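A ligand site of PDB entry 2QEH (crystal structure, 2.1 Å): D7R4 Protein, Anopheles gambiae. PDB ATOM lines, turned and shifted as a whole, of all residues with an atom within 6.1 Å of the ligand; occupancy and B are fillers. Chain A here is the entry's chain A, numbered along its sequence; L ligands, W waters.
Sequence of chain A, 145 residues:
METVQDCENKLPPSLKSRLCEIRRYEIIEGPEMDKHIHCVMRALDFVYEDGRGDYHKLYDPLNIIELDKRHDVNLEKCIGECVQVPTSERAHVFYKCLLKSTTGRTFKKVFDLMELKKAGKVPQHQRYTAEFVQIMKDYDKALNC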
ATOM      1  N   VAL A   4       0.971 -21.785  -4.274  1.00  0.00           N
ATOM      2  CA  VAL A   4      -0.025 -21.348  -3.297  1.00  0.00           C
ATOM      3  C   VAL A   4       0.160 -22.099  -1.974  1.00  0.00           C
ATOM      4  O   VAL A   4      -0.007 -21.536  -0.885  1.00  0.00           O
ATOM      5  CB  VAL A   4      -1.460 -21.562  -3.826  1.00  0.00           C
ATOM      6  CG1 VAL A   4      -2.486 -21.273  -2.740  1.00  0.00           C
ATOM      7  CG2 VAL A   4      -1.722 -20.690  -5.087  1.00  0.00           C
ATOM      8  N   CYS A   7       2.868 -20.557  -0.058  1.00  0.00           N
ATOM      9  CA  CYS A   7       2.388 -19.370   0.623  1.00  0.00           C
ATOM     10  C   CYS A   7       1.601 -19.667   1.907  1.00  0.00           C
ATOM     11  O   CYS A   7       1.784 -18.995   2.922  1.00  0.00           O
ATOM     12  CB  CYS A   7       1.564 -18.455  -0.298  1.00  0.00           C
ATOM     13  SG  CYS A   7       2.382 -17.938  -1.825  1.00  0.00           S
ATOM     14  N   GLU A   8       0.709 -20.638   1.858  1.00  0.00           N
ATOM     15  CA  GLU A   8      -0.055 -21.010   3.044  1.00  0.00           C
ATOM     16  C   GLU A   8       0.824 -21.605   4.161  1.00  0.00           C
ATOM     17  O   GLU A   8       0.554 -21.404   5.347  1.00  0.00           O
ATOM     18  CB  GLU A   8      -1.197 -21.968   2.683  1.00  0.00           C
ATOM     19  CG  GLU A   8      -1.847 -21.649   1.344  1.00  0.00           C
ATOM     20  CD  GLU A   8      -3.129 -22.403   1.088  1.00  0.00           C
ATOM     21  OE1 GLU A   8      -3.161 -23.644   1.315  1.00  0.00           O
ATOM     22  OE2 GLU A   8      -4.104 -21.759   0.650  1.00  0.00           O
ATOM     23  N   LEU A  11       2.125 -18.840   6.272  1.00  0.00           N
ATOM     24  CA  LEU A  11       1.212 -17.949   6.972  1.00  0.00           C
ATOM     25  C   LEU A  11       1.575 -17.823   8.448  1.00  0.00           C
ATOM     26  O   LEU A  11       2.093 -18.769   9.050  1.00  0.00           O
ATOM     27  CB  LEU A  11      -0.233 -18.443   6.839  1.00  0.00           C
ATOM     28  CG  LEU A  11      -0.975 -18.034   5.560  1.00  0.00           C
ATOM     29  CD1 LEU A  11      -2.127 -18.981   5.276  1.00  0.00           C
ATOM     30  CD2 LEU A  11      -1.459 -16.599   5.665  1.00  0.00           C
ATOM     31  N   LEU A  19      -7.584 -20.531   7.582  1.00  0.00           N
ATOM     32  CA  LEU A  19      -7.277 -20.942   6.220  1.00  0.00           C
ATOM     33  C   LEU A  19      -8.525 -21.176   5.374  1.00  0.00           C
ATOM     34  O   LEU A  19      -8.524 -20.874   4.186  1.00  0.00           O
ATOM     35  CB  LEU A  19      -6.394 -22.194   6.205  1.00  0.00           C
ATOM     36  CG  LEU A  19      -5.976 -22.648   4.801  1.00  0.00           C
ATOM     37  CD1 LEU A  19      -5.041 -21.641   4.157  1.00  0.00           C
ATOM     38  CD2 LEU A  19      -5.342 -24.026   4.802  1.00  0.00           C
ATOM     39  N   ILE A  22     -10.139 -17.970   4.148  1.00  0.00           N
ATOM     40  CA  ILE A  22      -9.264 -17.542   3.055  1.00  0.00           C
ATOM     41  C   ILE A  22      -9.588 -18.300   1.750  1.00  0.00           C
ATOM     42  O   ILE A  22      -9.813 -17.691   0.705  1.00  0.00           O
ATOM     43  CB  ILE A  22      -7.802 -17.767   3.462  1.00  0.00           C
ATOM     44  CG1 ILE A  22      -7.494 -17.007   4.751  1.00  0.00           C
ATOM     45  CG2 ILE A  22      -6.839 -17.384   2.331  1.00  0.00           C
ATOM     46  CD1 ILE A  22      -6.015 -16.952   5.077  1.00  0.00           C
ATOM     47  N   ARG A  23      -9.619 -19.632   1.812  1.00  0.00           N
ATOM     48  CA  ARG A  23      -9.795 -20.461   0.618  1.00  0.00           C
ATOM     49  C   ARG A  23     -11.249 -20.490   0.124  1.00  0.00           C
ATOM     50  O   ARG A  23     -11.539 -21.098  -0.912  1.00  0.00           O
ATOM     51  CB  ARG A  23      -9.251 -21.886   0.862  1.00  0.00           C
ATOM     52  CG  ARG A  23      -7.738 -21.947   1.063  1.00  0.00           C
ATOM     53  CD  ARG A  23      -7.219 -23.403   1.197  1.00  0.00           C
ATOM     54  NE  ARG A  23      -7.506 -24.158  -0.018  1.00  0.00           N
ATOM     55  CZ  ARG A  23      -6.784 -24.092  -1.134  1.00  0.00           C
ATOM     56  NH1 ARG A  23      -5.702 -23.331  -1.182  1.00  0.00           N
ATOM     57  NH2 ARG A  23      -7.141 -24.795  -2.186  1.00  0.00           N
ATOM     58  N   ARG A  24     -12.150 -19.844   0.859  1.00  0.00           N
ATOM     59  CA  ARG A  24     -13.530 -19.610   0.406  1.00  0.00           C
ATOM     60  C   ARG A  24     -13.652 -18.244  -0.282  1.00  0.00           C
ATOM     61  O   ARG A  24     -14.758 -17.803  -0.596  1.00  0.00           O
ATOM     62  CB  ARG A  24     -14.516 -19.647   1.595  1.00  0.00           C
ATOM     63  CG  ARG A  24     -14.836 -21.042   2.103  1.00  0.00           C
ATOM     64  CD  ARG A  24     -16.072 -21.043   2.994  1.00  0.00           C
ATOM     65  NE  ARG A  24     -15.987 -20.108   4.112  1.00  0.00           N
ATOM     66  CZ  ARG A  24     -15.586 -20.424   5.347  1.00  0.00           C
ATOM     67  NH1 ARG A  24     -15.216 -21.667   5.627  1.00  0.00           N
ATOM     68  NH2 ARG A  24     -15.544 -19.502   6.296  1.00  0.00           N
ATOM     69  N   TYR A  25     -12.510 -17.600  -0.523  1.00  0.00           N
ATOM     70  CA  TYR A  25     -12.455 -16.242  -1.096  1.00  0.00           C
ATOM     71  C   TYR A  25     -13.066 -15.203  -0.162  1.00  0.00           C
ATOM     72  O   TYR A  25     -13.462 -14.110  -0.590  1.00  0.00           O
ATOM     73  CB  TYR A  25     -13.128 -16.179  -2.462  1.00  0.00           C
ATOM     74  CG  TYR A  25     -12.464 -17.035  -3.523  1.00  0.00           C
ATOM     75  CD1 TYR A  25     -11.413 -16.534  -4.291  1.00  0.00           C
ATOM     76  CD2 TYR A  25     -12.878 -18.347  -3.740  1.00  0.00           C
ATOM     77  CE1 TYR A  25     -10.806 -17.313  -5.259  1.00  0.00           C
ATOM     78  CE2 TYR A  25     -12.260 -19.143  -4.706  1.00  0.00           C
ATOM     79  CZ  TYR A  25     -11.226 -18.616  -5.463  1.00  0.00           C
ATOM     80  OH  TYR A  25     -10.620 -19.395  -6.416  1.00  0.00           O
ATOM     81  N   MET A  33      -2.621 -10.241   5.491  1.00  0.00           N
ATOM     82  CA  MET A  33      -3.358 -10.693   4.326  1.00  0.00           C
ATOM     83  C   MET A  33      -2.862 -10.041   3.042  1.00  0.00           C
ATOM     84  O   MET A  33      -2.958 -10.635   1.961  1.00  0.00           O
ATOM     85  CB  MET A  33      -4.857 -10.449   4.521  1.00  0.00           C
ATOM     86  CG  MET A  33      -5.551 -11.554   5.303  1.00  0.00           C
ATOM     87  SD  MET A  33      -5.323 -13.155   4.469  1.00  0.00           S
ATOM     88  CE  MET A  33      -6.629 -13.067   3.255  1.00  0.00           C
ATOM     89  N   HIS A  36       0.202 -12.138   2.019  1.00  0.00           N
ATOM     90  CA  HIS A  36      -0.190 -13.484   1.611  1.00  0.00           C
ATOM     91  C   HIS A  36      -0.824 -13.514   0.221  1.00  0.00           C
ATOM     92  O   HIS A  36      -0.471 -14.336  -0.624  1.00  0.00           O
ATOM     93  CB  HIS A  36      -1.156 -14.106   2.618  1.00  0.00           C
ATOM     94  CG  HIS A  36      -1.652 -15.462   2.233  1.00  0.00           C
ATOM     95  ND1 HIS A  36      -0.804 -16.547   2.079  1.00  0.00           N
ATOM     96  CD2 HIS A  36      -2.898 -15.911   1.949  1.00  0.00           C
ATOM     97  CE1 HIS A  36      -1.519 -17.611   1.725  1.00  0.00           C
ATOM     98  NE2 HIS A  36      -2.786 -17.245   1.638  1.00  0.00           N
ATOM     99  N   ILE A  37      -1.763 -12.596  -0.002  1.00  0.00           N
ATOM    100  CA  ILE A  37      -2.440 -12.461  -1.283  1.00  0.00           C
ATOM    101  C   ILE A  37      -1.526 -11.991  -2.419  1.00  0.00           C
ATOM    102  O   ILE A  37      -1.760 -12.322  -3.573  1.00  0.00           O
ATOM    103  CB  ILE A  37      -3.677 -11.561  -1.175  1.00  0.00           C
ATOM    104  CG1 ILE A  37      -4.694 -12.180  -0.225  1.00  0.00           C
ATOM    105  CG2 ILE A  37      -4.315 -11.353  -2.563  1.00  0.00           C
ATOM    106  CD1 ILE A  37      -5.020 -13.609  -0.538  1.00  0.00           C
ATOM    107  N   VAL A  40       0.172 -15.364  -3.251  1.00  0.00           N
ATOM    108  CA  VAL A  40      -0.649 -16.254  -4.082  1.00  0.00           C
ATOM    109  C   VAL A  40      -0.952 -15.723  -5.488  1.00  0.00           C
ATOM    110  O   VAL A  40      -0.866 -16.461  -6.460  1.00  0.00           O
ATOM    111  CB  VAL A  40      -1.916 -16.789  -3.386  1.00  0.00           C
ATOM    112  CG1 VAL A  40      -1.629 -17.212  -1.953  1.00  0.00           C
ATOM    113  CG2 VAL A  40      -3.061 -15.816  -3.472  1.00  0.00           C
ATOM    114  N   TYR A  95      -7.308  -8.176  -6.178  1.00  0.00           N
ATOM    115  CA  TYR A  95      -8.028  -9.394  -5.865  1.00  0.00           C
ATOM    116  C   TYR A  95      -9.390  -9.059  -5.265  1.00  0.00           C
ATOM    117  O   TYR A  95     -10.437  -9.503  -5.758  1.00  0.00           O
ATOM    118  CB  TYR A  95      -7.132 -10.185  -4.904  1.00  0.00           C
ATOM    119  CG  TYR A  95      -7.729 -11.365  -4.167  1.00  0.00           C
ATOM    120  CD1 TYR A  95      -7.660 -12.644  -4.690  1.00  0.00           C
ATOM    121  CD2 TYR A  95      -8.312 -11.185  -2.930  1.00  0.00           C
ATOM    122  CE1 TYR A  95      -8.183 -13.740  -3.999  1.00  0.00           C
ATOM    123  CE2 TYR A  95      -8.838 -12.247  -2.239  1.00  0.00           C
ATOM    124  CZ  TYR A  95      -8.769 -13.527  -2.763  1.00  0.00           C
ATOM    125  OH  TYR A  95      -9.301 -14.569  -2.051  1.00  0.00           O
ATOM    126  N   LYS A 108     -13.160 -16.733  -9.662  1.00  0.00           N
ATOM    127  CA  LYS A 108     -12.949 -17.875  -8.760  1.00  0.00           C
ATOM    128  C   LYS A 108     -12.768 -19.199  -9.504  1.00  0.00           C
ATOM    129  O   LYS A 108     -12.007 -20.054  -9.075  1.00  0.00           O
ATOM    130  CB  LYS A 108     -14.116 -17.980  -7.768  1.00  0.00           C
ATOM    131  CG  LYS A 108     -14.181 -16.805  -6.781  1.00  0.00           C
ATOM    132  CD  LYS A 108     -15.373 -16.936  -5.799  1.00  0.00           C
ATOM    133  CE  LYS A 108     -16.648 -16.344  -6.399  1.00  0.00           C
ATOM    134  NZ  LYS A 108     -17.875 -16.549  -5.565  1.00  0.00           N
ATOM    135  N   PHE A 111      -9.244 -18.860 -11.043  1.00  0.00           N
ATOM    136  CA  PHE A 111      -8.334 -19.024  -9.904  1.00  0.00           C
ATOM    137  C   PHE A 111      -8.232 -20.510  -9.469  1.00  0.00           C
ATOM    138  O   PHE A 111      -7.132 -21.048  -9.363  1.00  0.00           O
ATOM    139  CB  PHE A 111      -8.833 -18.116  -8.770  1.00  0.00           C
ATOM    140  CG  PHE A 111      -7.902 -18.013  -7.583  1.00  0.00           C
ATOM    141  CD1 PHE A 111      -7.663 -19.111  -6.769  1.00  0.00           C
ATOM    142  CD2 PHE A 111      -7.309 -16.801  -7.250  1.00  0.00           C
ATOM    143  CE1 PHE A 111      -6.827 -19.009  -5.658  1.00  0.00           C
ATOM    144  CE2 PHE A 111      -6.481 -16.681  -6.154  1.00  0.00           C
ATOM    145  CZ  PHE A 111      -6.247 -17.794  -5.356  1.00  0.00           C
ATOM    146  N   ASP A 112      -9.371 -21.162  -9.213  1.00  0.00           N
ATOM    147  CA  ASP A 112      -9.352 -22.585  -8.852  1.00  0.00           C
ATOM    148  C   ASP A 112      -8.592 -23.410  -9.900  1.00  0.00           C
ATOM    149  O   ASP A 112      -7.709 -24.215  -9.562  1.00  0.00           O
ATOM    150  CB  ASP A 112     -10.774 -23.161  -8.697  1.00  0.00           C
ATOM    151  CG  ASP A 112     -11.462 -22.726  -7.401  1.00  0.00           C
ATOM    152  OD1 ASP A 112     -10.847 -22.041  -6.549  1.00  0.00           O
ATOM    153  OD2 ASP A 112     -12.648 -23.089  -7.227  1.00  0.00           O
ATOM    154  N   GLU A 115      -4.911 -22.893  -9.876  1.00  0.00           N
ATOM    155  CA  GLU A 115      -4.266 -23.373  -8.667  1.00  0.00           C
ATOM    156  C   GLU A 115      -3.962 -24.853  -8.826  1.00  0.00           C
ATOM    157  O   GLU A 115      -2.856 -25.306  -8.519  1.00  0.00           O
ATOM    158  CB  GLU A 115      -5.154 -23.146  -7.442  1.00  0.00           C
ATOM    159  CG  GLU A 115      -4.465 -23.513  -6.120  1.00  0.00           C
ATOM    160  CD  GLU A 115      -5.432 -23.679  -4.966  1.00  0.00           C
ATOM    161  OE1 GLU A 115      -6.660 -23.516  -5.157  1.00  0.00           O
ATOM    162  OE2 GLU A 115      -4.967 -23.978  -3.844  1.00  0.00           O
ATOM    163  N   MET A 136     -11.818 -30.112  -6.661  1.00  0.00           N
ATOM    164  CA  MET A 136     -11.469 -28.980  -5.826  1.00  0.00           C
ATOM    165  C   MET A 136     -11.948 -29.211  -4.380  1.00  0.00           C
ATOM    166  O   MET A 136     -11.218 -28.938  -3.438  1.00  0.00           O
ATOM    167  CB  MET A 136     -12.044 -27.677  -6.418  1.00  0.00           C
ATOM    168  CG  MET A 136     -11.648 -26.400  -5.691  1.00  0.00           C
ATOM    169  SD  MET A 136      -9.933 -25.827  -5.935  1.00  0.00           S
ATOM    170  CE  MET A 136      -9.246 -26.376  -4.393  1.00  0.00           C
ATOM    171  N   ASP A 140      -9.545 -29.431  -1.030  1.00  0.00           N
ATOM    172  CA  ASP A 140      -9.745 -28.617   0.164  1.00  0.00           C
ATOM    173  C   ASP A 140      -9.977 -29.503   1.387  1.00  0.00           C
ATOM    174  O   ASP A 140      -9.508 -29.195   2.473  1.00  0.00           O
ATOM    175  CB  ASP A 140     -10.945 -27.681  -0.023  1.00  0.00           C
ATOM    176  CG  ASP A 140     -10.599 -26.417  -0.836  1.00  0.00           C
ATOM    177  OD1 ASP A 140      -9.398 -26.138  -1.023  1.00  0.00           O
ATOM    178  OD2 ASP A 140     -11.527 -25.737  -1.295  1.00  0.00           O
HETATM  179  O1  LIG L   1      -3.925 -19.192  -0.208  1.00  0.00           O
HETATM  180  C1  LIG L   1      -5.081 -18.725  -0.743  1.00  0.00           C
HETATM  181  C2  LIG L   1      -5.308 -17.345  -0.668  1.00  0.00           C
HETATM  182  C3  LIG L   1      -6.470 -16.824  -1.210  1.00  0.00           C
HETATM  183  C4  LIG L   1      -7.340 -17.714  -1.805  1.00  0.00           C
HETATM  184  N1  LIG L   1      -8.546 -17.565  -2.399  1.00  0.00           N
HETATM  185  C5  LIG L   1      -8.989 -18.779  -2.805  1.00  0.00           C
HETATM  186  C6  LIG L   1      -8.046 -19.745  -2.474  1.00  0.00           C
HETATM  187  C7  LIG L   1      -7.023 -19.064  -1.825  1.00  0.00           C
HETATM  188  C8  LIG L   1      -5.926 -19.532  -1.327  1.00  0.00           C
HETATM  189  C9  LIG L   1      -8.204 -21.228  -2.773  1.00  0.00           C
HETATM  190  C10 LIG L   1      -9.120 -21.406  -4.002  1.00  0.00           C
HETATM  191  N2  LIG L   1      -9.189 -22.802  -4.410  1.00  0.00           N
HETATM  192  O   HOH W   1     -10.933 -23.554  -2.452  1.00  0.00           O
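OE2 of Glu 8 sits at hydrogen-bond distance from O1 of the ligand (2.7 Å).
N2 of the ligand is in salt-bridge range of OE1 of Glu 115, 2.7 Å away.
OD1 of Asp 112 lies within salt-bridge range of N2 of the ligand (2.8 Å).
O1 of the ligand sits at hydrogen-bond distance from NE2 of His 36 (2.9 Å).
The side-chain hydroxyl of Tyr 95 sits at hydrogen-bond distance from a nitrogen (N1) of the ligand.
A nitrogen (N1) of the ligand lies within hydrogen-bond range of the backbone carbonyl oxygen (O) of Ile 22 (3.4 Å).
N2 of the ligand lies within hydrogen-bond range of SD of Met 136 (3.5 Å).
The side-chain carboxylate of Glu 8 is in salt-bridge range of the guanidinium group of Arg 23.
The side-chain carboxylate (OE2) of Glu 115 is in salt-bridge range of the guanidinium group (NH1) of Arg 23 (2.8 Å).
The side-chain carboxylate of Asp 112 is in hydrogen-bond range of the side-chain hydroxyl of Tyr 25 (2.7 Å).
The side-chain hydroxyl (OH) of Tyr 25 sits at hydrogen-bond distance from the backbone carbonyl oxygen (O) of Lys 108 (3.1 Å).
N of Val 40 sits at hydrogen-bond distance from SG of Cys 7 (3.7 Å).
The guanidinium group (NH2) of Arg 23 is in salt-bridge range of the side-chain carboxylate (OD1) of Asp 140 (2.9 Å).
Water W1 lies within hydrogen-bond range of OD2 of Asp 140 (2.5 Å), N2 of the ligand (2.7 Å) and O of Arg 23 (3.0 Å).
Merely in contact with the ligand: Val 4 (3.6 Å), Arg 23 (3.6 Å), Tyr 25 (3.4 Å), Ile 37 (3.6 Å), Val 40 (3.5 Å) and Phe 111 (3.5 Å).
Hydrophobic or aromatic side chains within 4 Å of the ligand: Val 4, Ile 22, Tyr 25, His 36, Ile 37, Val 40, Phe 111 and Met 136.
13 residues have an atom within 4 Å of the ligand: Val 4, Glu 8, Ile 22, Arg 23, Tyr 25, His 36, Ile 37, Val 40, Tyr 95, Phe 111, Asp 112, Glu 115 and Met 136.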
